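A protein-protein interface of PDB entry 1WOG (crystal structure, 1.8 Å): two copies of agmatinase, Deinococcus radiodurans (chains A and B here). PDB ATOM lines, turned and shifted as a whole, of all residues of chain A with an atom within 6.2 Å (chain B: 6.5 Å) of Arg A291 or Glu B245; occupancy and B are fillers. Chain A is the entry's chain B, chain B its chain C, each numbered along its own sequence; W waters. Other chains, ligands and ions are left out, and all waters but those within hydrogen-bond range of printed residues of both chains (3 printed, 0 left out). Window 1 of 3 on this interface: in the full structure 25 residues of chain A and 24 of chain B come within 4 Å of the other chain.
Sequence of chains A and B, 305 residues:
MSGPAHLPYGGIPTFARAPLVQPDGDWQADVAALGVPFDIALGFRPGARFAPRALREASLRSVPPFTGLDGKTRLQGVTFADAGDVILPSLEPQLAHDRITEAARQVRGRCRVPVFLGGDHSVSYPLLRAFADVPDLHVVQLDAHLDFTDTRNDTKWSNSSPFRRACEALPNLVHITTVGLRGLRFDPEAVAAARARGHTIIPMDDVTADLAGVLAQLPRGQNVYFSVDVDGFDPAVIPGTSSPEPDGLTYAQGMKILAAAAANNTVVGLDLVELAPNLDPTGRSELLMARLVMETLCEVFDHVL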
ATOM      1  N   ALA A  58     -13.979   5.553 -20.495  1.00  0.00           N
ATOM      2  CA  ALA A  58     -15.221   5.094 -19.888  1.00  0.00           C
ATOM      3  C   ALA A  58     -15.775   3.853 -20.589  1.00  0.00           C
ATOM      4  O   ALA A  58     -16.390   3.000 -19.950  1.00  0.00           O
ATOM      5  CB  ALA A  58     -16.262   6.217 -19.910  1.00  0.00           C
ATOM      6  N   SER A  59     -15.553   3.751 -21.898  1.00  0.00           N
ATOM      7  CA  SER A  59     -16.058   2.611 -22.664  1.00  0.00           C
ATOM      8  C   SER A  59     -15.401   1.297 -22.253  1.00  0.00           C
ATOM      9  O   SER A  59     -15.908   0.224 -22.575  1.00  0.00           O
ATOM     10  CB  SER A  59     -15.858   2.832 -24.169  1.00  0.00           C
ATOM     11  OG  SER A  59     -14.497   2.688 -24.537  1.00  0.00           O
ATOM     12  N   SER A  62     -17.603  -0.808 -20.797  1.00  0.00           N
ATOM     13  CA  SER A  62     -18.635  -1.329 -21.692  1.00  0.00           C
ATOM     14  C   SER A  62     -18.082  -2.020 -22.936  1.00  0.00           C
ATOM     15  O   SER A  62     -18.408  -1.634 -24.059  1.00  0.00           O
ATOM     16  CB  SER A  62     -19.567  -0.197 -22.134  1.00  0.00           C
ATOM     17  OG  SER A  62     -20.231   0.395 -21.029  1.00  0.00           O
ATOM     18  N   TYR A 251     -31.678   8.958 -18.115  1.00  0.00           N
ATOM     19  CA  TYR A 251     -30.933   8.095 -19.015  1.00  0.00           C
ATOM     20  C   TYR A 251     -31.938   7.190 -19.746  1.00  0.00           C
ATOM     21  O   TYR A 251     -31.890   7.041 -20.973  1.00  0.00           O
ATOM     22  CB  TYR A 251     -29.949   7.234 -18.218  1.00  0.00           C
ATOM     23  CG  TYR A 251     -29.159   6.269 -19.072  1.00  0.00           C
ATOM     24  CD1 TYR A 251     -27.874   6.587 -19.511  1.00  0.00           C
ATOM     25  CD2 TYR A 251     -29.715   5.052 -19.478  1.00  0.00           C
ATOM     26  CE1 TYR A 251     -27.161   5.717 -20.337  1.00  0.00           C
ATOM     27  CE2 TYR A 251     -29.014   4.182 -20.304  1.00  0.00           C
ATOM     28  CZ  TYR A 251     -27.740   4.522 -20.730  1.00  0.00           C
ATOM     29  OH  TYR A 251     -27.052   3.672 -21.560  1.00  0.00           O
ATOM     30  N   MET A 255     -32.687   6.794 -23.793  1.00  0.00           N
ATOM     31  CA  MET A 255     -32.419   5.481 -24.371  1.00  0.00           C
ATOM     32  C   MET A 255     -33.663   4.884 -25.028  1.00  0.00           C
ATOM     33  O   MET A 255     -33.561   4.206 -26.052  1.00  0.00           O
ATOM     34  CB  MET A 255     -31.877   4.535 -23.293  1.00  0.00           C
ATOM     35  CG  MET A 255     -31.158   3.303 -23.833  1.00  0.00           C
ATOM     36  SD  MET A 255     -29.788   3.708 -24.962  1.00  0.00           S
ATOM     37  CE  MET A 255     -30.394   2.934 -26.488  1.00  0.00           C
ATOM     38  N   GLU A 286     -19.199  10.738 -18.166  1.00  0.00           N
ATOM     39  CA  GLU A 286     -18.568   9.963 -19.230  1.00  0.00           C
ATOM     40  C   GLU A 286     -18.919   8.476 -19.131  1.00  0.00           C
ATOM     41  O   GLU A 286     -19.121   7.810 -20.145  1.00  0.00           O
ATOM     42  CB  GLU A 286     -17.046  10.142 -19.211  1.00  0.00           C
ATOM     43  CG  GLU A 286     -16.390   9.899 -17.870  1.00  0.00           C
ATOM     44  CD  GLU A 286     -16.074  11.196 -17.161  1.00  0.00           C
ATOM     45  OE1 GLU A 286     -14.882  11.433 -16.876  1.00  0.00           O
ATOM     46  OE2 GLU A 286     -17.012  11.980 -16.895  1.00  0.00           O
ATOM     47  N   LEU A 287     -19.004   7.951 -17.916  1.00  0.00           N
ATOM     48  CA  LEU A 287     -19.342   6.541 -17.757  1.00  0.00           C
ATOM     49  C   LEU A 287     -20.717   6.226 -18.343  1.00  0.00           C
ATOM     50  O   LEU A 287     -20.884   5.248 -19.080  1.00  0.00           O
ATOM     51  CB  LEU A 287     -19.303   6.139 -16.276  1.00  0.00           C
ATOM     52  CG  LEU A 287     -17.906   6.039 -15.652  1.00  0.00           C
ATOM     53  CD1 LEU A 287     -18.020   5.738 -14.168  1.00  0.00           C
ATOM     54  CD2 LEU A 287     -17.113   4.942 -16.348  1.00  0.00           C
ATOM     55  N   LEU A 288     -21.701   7.060 -18.017  1.00  0.00           N
ATOM     56  CA  LEU A 288     -23.058   6.845 -18.501  1.00  0.00           C
ATOM     57  C   LEU A 288     -23.202   7.107 -19.990  1.00  0.00           C
ATOM     58  O   LEU A 288     -23.949   6.409 -20.672  1.00  0.00           O
ATOM     59  CB  LEU A 288     -24.047   7.726 -17.730  1.00  0.00           C
ATOM     60  CG  LEU A 288     -24.657   7.138 -16.451  1.00  0.00           C
ATOM     61  CD1 LEU A 288     -23.569   6.634 -15.508  1.00  0.00           C
ATOM     62  CD2 LEU A 288     -25.504   8.211 -15.771  1.00  0.00           C
ATOM     63  N   MET A 289     -22.493   8.108 -20.504  1.00  0.00           N
ATOM     64  CA  MET A 289     -22.604   8.411 -21.927  1.00  0.00           C
ATOM     65  C   MET A 289     -21.868   7.404 -22.800  1.00  0.00           C
ATOM     66  O   MET A 289     -22.269   7.161 -23.941  1.00  0.00           O
ATOM     67  CB  MET A 289     -22.136   9.841 -22.207  1.00  0.00           C
ATOM     68  CG  MET A 289     -23.101  10.905 -21.658  1.00  0.00           C
ATOM     69  SD  MET A 289     -24.776  10.852 -22.395  1.00  0.00           S
ATOM     70  CE  MET A 289     -25.642   9.691 -21.336  1.00  0.00           C
ATOM     71  N   ALA A 290     -20.801   6.807 -22.274  1.00  0.00           N
ATOM     72  CA  ALA A 290     -20.085   5.792 -23.037  1.00  0.00           C
ATOM     73  C   ALA A 290     -21.042   4.609 -23.126  1.00  0.00           C
ATOM     74  O   ALA A 290     -21.172   3.976 -24.179  1.00  0.00           O
ATOM     75  CB  ALA A 290     -18.801   5.379 -22.323  1.00  0.00           C
ATOM     76  N   ARG A 291     -21.726   4.321 -22.018  1.00  0.00           N
ATOM     77  CA  ARG A 291     -22.678   3.220 -21.998  1.00  0.00           C
ATOM     78  C   ARG A 291     -23.830   3.498 -22.960  1.00  0.00           C
ATOM     79  O   ARG A 291     -24.317   2.584 -23.635  1.00  0.00           O
ATOM     80  CB  ARG A 291     -23.259   2.996 -20.598  1.00  0.00           C
ATOM     81  CG  ARG A 291     -24.343   1.925 -20.622  1.00  0.00           C
ATOM     82  CD  ARG A 291     -25.126   1.781 -19.337  1.00  0.00           C
ATOM     83  NE  ARG A 291     -26.467   1.280 -19.638  1.00  0.00           N
ATOM     84  CZ  ARG A 291     -27.270   0.688 -18.762  1.00  0.00           C
ATOM     85  NH1 ARG A 291     -26.876   0.501 -17.509  1.00  0.00           N
ATOM     86  NH2 ARG A 291     -28.485   0.304 -19.138  1.00  0.00           N
ATOM     87  N   LEU A 292     -24.264   4.754 -23.016  1.00  0.00           N
ATOM     88  CA  LEU A 292     -25.359   5.136 -23.899  1.00  0.00           C
ATOM     89  C   LEU A 292     -25.031   4.745 -25.332  1.00  0.00           C
ATOM     90  O   LEU A 292     -25.866   4.171 -26.035  1.00  0.00           O
ATOM     91  CB  LEU A 292     -25.605   6.646 -23.853  1.00  0.00           C
ATOM     92  CG  LEU A 292     -26.851   7.096 -24.628  1.00  0.00           C
ATOM     93  CD1 LEU A 292     -28.089   6.774 -23.803  1.00  0.00           C
ATOM     94  CD2 LEU A 292     -26.793   8.590 -24.928  1.00  0.00           C
ATOM     95  N   VAL A 293     -23.813   5.067 -25.761  1.00  0.00           N
ATOM     96  CA  VAL A 293     -23.383   4.754 -27.118  1.00  0.00           C
ATOM     97  C   VAL A 293     -23.414   3.249 -27.355  1.00  0.00           C
ATOM     98  O   VAL A 293     -23.952   2.786 -28.357  1.00  0.00           O
ATOM     99  CB  VAL A 293     -21.954   5.292 -27.400  1.00  0.00           C
ATOM    100  CG1 VAL A 293     -21.502   4.876 -28.793  1.00  0.00           C
ATOM    101  CG2 VAL A 293     -21.939   6.807 -27.287  1.00  0.00           C
ATOM    102  N   MET A 294     -22.855   2.481 -26.423  1.00  0.00           N
ATOM    103  CA  MET A 294     -22.836   1.034 -26.580  1.00  0.00           C
ATOM    104  C   MET A 294     -24.233   0.412 -26.591  1.00  0.00           C
ATOM    105  O   MET A 294     -24.507  -0.481 -27.398  1.00  0.00           O
ATOM    106  CB  MET A 294     -21.976   0.390 -25.489  1.00  0.00           C
ATOM    107  CG  MET A 294     -20.499   0.776 -25.563  1.00  0.00           C
ATOM    108  SD  MET A 294     -19.726   0.427 -27.173  1.00  0.00           S
ATOM    109  CE  MET A 294     -19.951  -1.352 -27.264  1.00  0.00           C
ATOM    110  N   GLU A 295     -25.117   0.875 -25.708  1.00  0.00           N
ATOM    111  CA  GLU A 295     -26.476   0.339 -25.656  1.00  0.00           C
ATOM    112  C   GLU A 295     -27.226   0.691 -26.942  1.00  0.00           C
ATOM    113  O   GLU A 295     -28.022  -0.104 -27.436  1.00  0.00           O
ATOM    114  CB  GLU A 295     -27.236   0.874 -24.426  1.00  0.00           C
ATOM    115  CG  GLU A 295     -28.659   0.314 -24.268  1.00  0.00           C
ATOM    116  CD  GLU A 295     -29.300   0.647 -22.922  1.00  0.00           C
ATOM    117  OE1 GLU A 295     -30.474   0.267 -22.708  1.00  0.00           O
ATOM    118  OE2 GLU A 295     -28.636   1.285 -22.078  1.00  0.00           O
ATOM    119  N   THR A 296     -26.966   1.877 -27.489  1.00  0.00           N
ATOM    120  CA  THR A 296     -27.624   2.279 -28.725  1.00  0.00           C
ATOM    121  C   THR A 296     -27.193   1.312 -29.829  1.00  0.00           C
ATOM    122  O   THR A 296     -28.010   0.871 -30.643  1.00  0.00           O
ATOM    123  CB  THR A 296     -27.255   3.728 -29.113  1.00  0.00           C
ATOM    124  OG1 THR A 296     -27.780   4.633 -28.129  1.00  0.00           O
ATOM    125  CG2 THR A 296     -27.848   4.090 -30.473  1.00  0.00           C
ATOM    126  N   ALA B 144     -26.895  -2.852  -7.792  1.00  0.00           N
ATOM    127  CA  ALA B 144     -27.128  -2.766  -9.228  1.00  0.00           C
ATOM    128  C   ALA B 144     -26.565  -4.065  -9.807  1.00  0.00           C
ATOM    129  O   ALA B 144     -26.879  -4.452 -10.933  1.00  0.00           O
ATOM    130  CB  ALA B 144     -26.388  -1.569  -9.819  1.00  0.00           C
ATOM    131  N   HIS B 145     -25.732  -4.737  -9.015  1.00  0.00           N
ATOM    132  CA  HIS B 145     -25.094  -5.980  -9.449  1.00  0.00           C
ATOM    133  C   HIS B 145     -25.483  -7.171  -8.567  1.00  0.00           C
ATOM    134  O   HIS B 145     -25.780  -7.005  -7.386  1.00  0.00           O
ATOM    135  CB  HIS B 145     -23.574  -5.813  -9.435  1.00  0.00           C
ATOM    136  CG  HIS B 145     -23.105  -4.488  -9.955  1.00  0.00           C
ATOM    137  ND1 HIS B 145     -23.062  -3.352  -9.173  1.00  0.00           N
ATOM    138  CD2 HIS B 145     -22.662  -4.119 -11.180  1.00  0.00           C
ATOM    139  CE1 HIS B 145     -22.611  -2.341  -9.895  1.00  0.00           C
ATOM    140  NE2 HIS B 145     -22.360  -2.779 -11.116  1.00  0.00           N
ATOM    141  N   ARG B 182     -29.455  -3.941 -12.693  1.00  0.00           N
ATOM    142  CA  ARG B 182     -29.541  -3.250 -13.968  1.00  0.00           C
ATOM    143  C   ARG B 182     -28.163  -3.210 -14.606  1.00  0.00           C
ATOM    144  O   ARG B 182     -27.154  -3.447 -13.941  1.00  0.00           O
ATOM    145  CB  ARG B 182     -30.067  -1.829 -13.761  1.00  0.00           C
ATOM    146  CG  ARG B 182     -29.234  -0.988 -12.800  1.00  0.00           C
ATOM    147  CD  ARG B 182     -29.955   0.305 -12.453  1.00  0.00           C
ATOM    148  NE  ARG B 182     -29.102   1.253 -11.738  1.00  0.00           N
ATOM    149  CZ  ARG B 182     -28.876   1.241 -10.428  1.00  0.00           C
ATOM    150  NH1 ARG B 182     -29.437   0.323  -9.649  1.00  0.00           N
ATOM    151  NH2 ARG B 182     -28.086   2.164  -9.894  1.00  0.00           N
ATOM    152  N   GLY B 183     -28.118  -2.917 -15.901  1.00  0.00           N
ATOM    153  CA  GLY B 183     -26.841  -2.865 -16.588  1.00  0.00           C
ATOM    154  C   GLY B 183     -26.845  -3.683 -17.862  1.00  0.00           C
ATOM    155  O   GLY B 183     -27.744  -4.501 -18.076  1.00  0.00           O
ATOM    156  N   LEU B 184     -25.837  -3.466 -18.703  1.00  0.00           N
ATOM    157  CA  LEU B 184     -25.723  -4.169 -19.977  1.00  0.00           C
ATOM    158  C   LEU B 184     -25.154  -5.571 -19.843  1.00  0.00           C
ATOM    159  O   LEU B 184     -25.487  -6.460 -20.629  1.00  0.00           O
ATOM    160  CB  LEU B 184     -24.836  -3.377 -20.944  1.00  0.00           C
ATOM    161  CG  LEU B 184     -25.330  -2.007 -21.412  1.00  0.00           C
ATOM    162  CD1 LEU B 184     -24.299  -1.386 -22.341  1.00  0.00           C
ATOM    163  CD2 LEU B 184     -26.669  -2.154 -22.116  1.00  0.00           C
ATOM    164  N   ASP B 231     -24.304   1.540  -4.755  1.00  0.00           N
ATOM    165  CA  ASP B 231     -24.546   1.720  -6.187  1.00  0.00           C
ATOM    166  C   ASP B 231     -25.911   1.204  -6.629  1.00  0.00           C
ATOM    167  O   ASP B 231     -26.265   1.279  -7.808  1.00  0.00           O
ATOM    168  CB  ASP B 231     -23.412   1.141  -7.070  1.00  0.00           C
ATOM    169  CG  ASP B 231     -23.305  -0.378  -7.032  1.00  0.00           C
ATOM    170  OD1 ASP B 231     -24.316  -1.087  -6.846  1.00  0.00           O
ATOM    171  OD2 ASP B 231     -22.174  -0.861  -7.228  1.00  0.00           O
ATOM    172  N   GLY B 232     -26.683   0.696  -5.674  1.00  0.00           N
ATOM    173  CA  GLY B 232     -28.030   0.252  -5.984  1.00  0.00           C
ATOM    174  C   GLY B 232     -28.846   1.515  -6.212  1.00  0.00           C
ATOM    175  O   GLY B 232     -29.831   1.521  -6.959  1.00  0.00           O
ATOM    176  N   PHE B 233     -28.418   2.601  -5.572  1.00  0.00           N
ATOM    177  CA  PHE B 233     -29.093   3.887  -5.705  1.00  0.00           C
ATOM    178  C   PHE B 233     -28.642   4.576  -6.985  1.00  0.00           C
ATOM    179  O   PHE B 233     -27.549   4.325  -7.489  1.00  0.00           O
ATOM    180  CB  PHE B 233     -28.792   4.789  -4.493  1.00  0.00           C
ATOM    181  CG  PHE B 233     -29.362   4.274  -3.198  1.00  0.00           C
ATOM    182  CD1 PHE B 233     -28.611   3.446  -2.371  1.00  0.00           C
ATOM    183  CD2 PHE B 233     -30.666   4.587  -2.827  1.00  0.00           C
ATOM    184  CE1 PHE B 233     -29.157   2.933  -1.184  1.00  0.00           C
ATOM    185  CE2 PHE B 233     -31.218   4.080  -1.645  1.00  0.00           C
ATOM    186  CZ  PHE B 233     -30.460   3.252  -0.825  1.00  0.00           C
ATOM    187  N   ASP B 234     -29.495   5.441  -7.511  1.00  0.00           N
ATOM    188  CA  ASP B 234     -29.191   6.164  -8.734  1.00  0.00           C
ATOM    189  C   ASP B 234     -27.939   7.016  -8.555  1.00  0.00           C
ATOM    190  O   ASP B 234     -27.760   7.667  -7.522  1.00  0.00           O
ATOM    191  CB  ASP B 234     -30.375   7.047  -9.118  1.00  0.00           C
ATOM    192  CG  ASP B 234     -30.303   7.529 -10.550  1.00  0.00           C
ATOM    193  OD1 ASP B 234     -29.540   8.474 -10.834  1.00  0.00           O
ATOM    194  OD2 ASP B 234     -31.010   6.948 -11.398  1.00  0.00           O
ATOM    195  N   PRO B 235     -27.051   7.007  -9.557  1.00  0.00           N
ATOM    196  CA  PRO B 235     -25.792   7.758  -9.571  1.00  0.00           C
ATOM    197  C   PRO B 235     -26.012   9.253  -9.347  1.00  0.00           C
ATOM    198  O   PRO B 235     -25.136   9.939  -8.826  1.00  0.00           O
ATOM    199  CB  PRO B 235     -25.235   7.478 -10.964  1.00  0.00           C
ATOM    200  CG  PRO B 235     -25.793   6.147 -11.307  1.00  0.00           C
ATOM    201  CD  PRO B 235     -27.196   6.201 -10.785  1.00  0.00           C
ATOM    202  N   THR B 241     -19.350   6.232  -5.814  1.00  0.00           N
ATOM    203  CA  THR B 241     -19.207   4.781  -5.828  1.00  0.00           C
ATOM    204  C   THR B 241     -18.386   4.384  -7.053  1.00  0.00           C
ATOM    205  O   THR B 241     -18.395   5.073  -8.074  1.00  0.00           O
ATOM    206  CB  THR B 241     -20.595   4.084  -5.826  1.00  0.00           C
ATOM    207  OG1 THR B 241     -20.437   2.702  -5.476  1.00  0.00           O
ATOM    208  CG2 THR B 241     -21.260   4.189  -7.195  1.00  0.00           C
ATOM    209  N   SER B 243     -18.507   1.790  -9.392  1.00  0.00           N
ATOM    210  CA  SER B 243     -19.165   1.422 -10.645  1.00  0.00           C
ATOM    211  C   SER B 243     -20.640   1.788 -10.726  1.00  0.00           C
ATOM    212  O   SER B 243     -21.506   0.935 -10.553  1.00  0.00           O
ATOM    213  CB  SER B 243     -19.010  -0.084 -10.859  1.00  0.00           C
ATOM    214  OG  SER B 243     -17.657  -0.472 -10.697  1.00  0.00           O
ATOM    215  N   PRO B 244     -20.943   3.062 -11.012  1.00  0.00           N
ATOM    216  CA  PRO B 244     -22.325   3.530 -11.115  1.00  0.00           C
ATOM    217  C   PRO B 244     -23.056   3.009 -12.351  1.00  0.00           C
ATOM    218  O   PRO B 244     -22.445   2.758 -13.393  1.00  0.00           O
ATOM    219  CB  PRO B 244     -22.169   5.047 -11.139  1.00  0.00           C
ATOM    220  CG  PRO B 244     -20.875   5.221 -11.883  1.00  0.00           C
ATOM    221  CD  PRO B 244     -19.993   4.165 -11.253  1.00  0.00           C
ATOM    222  N   GLU B 245     -24.365   2.845 -12.219  1.00  0.00           N
ATOM    223  CA  GLU B 245     -25.204   2.375 -13.314  1.00  0.00           C
ATOM    224  C   GLU B 245     -26.420   3.300 -13.318  1.00  0.00           C
ATOM    225  O   GLU B 245     -27.049   3.516 -12.283  1.00  0.00           O
ATOM    226  CB  GLU B 245     -25.620   0.920 -13.065  1.00  0.00           C
ATOM    227  CG  GLU B 245     -25.815   0.103 -14.329  1.00  0.00           C
ATOM    228  CD  GLU B 245     -24.573   0.062 -15.205  1.00  0.00           C
ATOM    229  OE1 GLU B 245     -23.570  -0.578 -14.822  1.00  0.00           O
ATOM    230  OE2 GLU B 245     -24.598   0.681 -16.282  1.00  0.00           O
ATOM    231  N   PRO B 246     -26.759   3.874 -14.481  1.00  0.00           N
ATOM    232  CA  PRO B 246     -27.912   4.778 -14.541  1.00  0.00           C
ATOM    233  C   PRO B 246     -29.248   4.163 -14.140  1.00  0.00           C
ATOM    234  O   PRO B 246     -29.407   2.937 -14.103  1.00  0.00           O
ATOM    235  CB  PRO B 246     -27.919   5.235 -16.000  1.00  0.00           C
ATOM    236  CG  PRO B 246     -27.383   4.027 -16.725  1.00  0.00           C
ATOM    237  CD  PRO B 246     -26.209   3.638 -15.829  1.00  0.00           C
ATOM    238  N   ASP B 247     -30.193   5.052 -13.841  1.00  0.00           N
ATOM    239  CA  ASP B 247     -31.556   4.702 -13.476  1.00  0.00           C
ATOM    240  C   ASP B 247     -31.666   3.725 -12.311  1.00  0.00           C
ATOM    241  O   ASP B 247     -32.174   2.609 -12.457  1.00  0.00           O
ATOM    242  CB  ASP B 247     -32.269   4.148 -14.712  1.00  0.00           C
ATOM    243  CG  ASP B 247     -32.121   5.057 -15.920  1.00  0.00           C
ATOM    244  OD1 ASP B 247     -32.618   6.207 -15.882  1.00  0.00           O
ATOM    245  OD2 ASP B 247     -31.497   4.626 -16.909  1.00  0.00           O
ATOM    246  N   GLY B 248     -31.200   4.167 -11.148  1.00  0.00           N
ATOM    247  CA  GLY B 248     -31.258   3.336  -9.966  1.00  0.00           C
ATOM    248  C   GLY B 248     -32.331   3.767  -8.990  1.00  0.00           C
ATOM    249  O   GLY B 248     -33.236   4.534  -9.320  1.00  0.00           O
HETATM  250  O   HOH W   1     -30.230  -1.704 -17.713  1.00  0.00           O
HETATM  251  O   HOH W   2     -31.214   8.632 -15.305  1.00  0.00           O
HETATM  252  O   HOH W   3     -29.298   0.732 -15.951  1.00  0.00           O
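The guanidinium group of Arg A291 lies within salt-bridge range of the side-chain carboxylate of Glu B245 (2.6 Å).
OH of Tyr A251 is in hydrogen-bond range of NE of Arg A291 (3.1 Å).
The side-chain hydroxyl (OH) of Tyr A251 sits close to the backbone NH (N) of Leu A292, 3.3 Å away.
The side-chain carboxylate (OE2) of Glu A295 lies within hydrogen-bond range of the side-chain hydroxyl (OH) of Tyr A251 (2.9 Å).
NH2 of Arg A291 is in salt-bridge range of OE2 of Glu A295 (3.1 Å).
The backbone carbonyl oxygen (O) of Asp B247 sits close to the guanidinium group (NE) of Arg B182 (3.4 Å).
The backbone NH (N) of Asp B247 sits close to the side-chain carboxylate (OD2) of Asp B234, 3.2 Å away.
Among the printed residues, pairs that only touch across the chains: Tyr A251 with Pro B246 (3.5 Å), Tyr A251 with Asp B247 (3.2 Å), Leu A287 with Pro B244 (3.7 Å), Leu A288 with Pro B246 (3.8 Å), Arg A291 with Gly B183 (3.5 Å), Arg A291 with Leu B184 (3.7 Å), Arg A291 with Pro B246 (3.6 Å) and Glu A295 with Leu B184 (3.8 Å).
Of chain B, only Gly B183 (3.5 Å), Leu B184 (3.7 Å), Glu B245 (2.6 Å) and Pro B246 (3.6 Å) come within 4 Å of Arg A291.
Met A294 touches none of the printed residues of chain B.
Printed residues of chain B within 4 Å of Glu A295: Leu B184.
Asp B234 touches none of the printed residues of chain A.
Of the printed residues of chain A, Glu B245 touches Arg A291 (2.6 Å).
Of the printed residues of chain A, Pro B246 touches Tyr A251, Leu A288 and Arg A291.
The nearest residue of chain A that does not touch Glu B245 is Leu A288 (4.9 Å).
Of the 16 printed residues of chain A, 5 touch a printed residue of chain B.
Printed residues of chain A that touch a printed residue of chain B: Tyr A251, Leu A287, Leu A288, Arg A291 and Glu A295.
Among the printed residues, Asp or Glu carboxylates within 4 Å of a Lys or Arg side-chain nitrogen of the other chain: Arg A291 with Glu B245 (2.6 Å).
No position is printed for both chains.
Water W2 bridges the side-chain carboxylate of Asp B247 (2.9 Å) and the backbone NH of Tyr A251 (2.9 Å).
Water W3 bridges O of Pro B246 (2.9 Å) and NH1 of Arg A291 (2.9 Å).
Water W1 lies within hydrogen-bond range of NH2 of Arg A291 (3.0 Å) and N of Gly B183 (3.0 Å).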
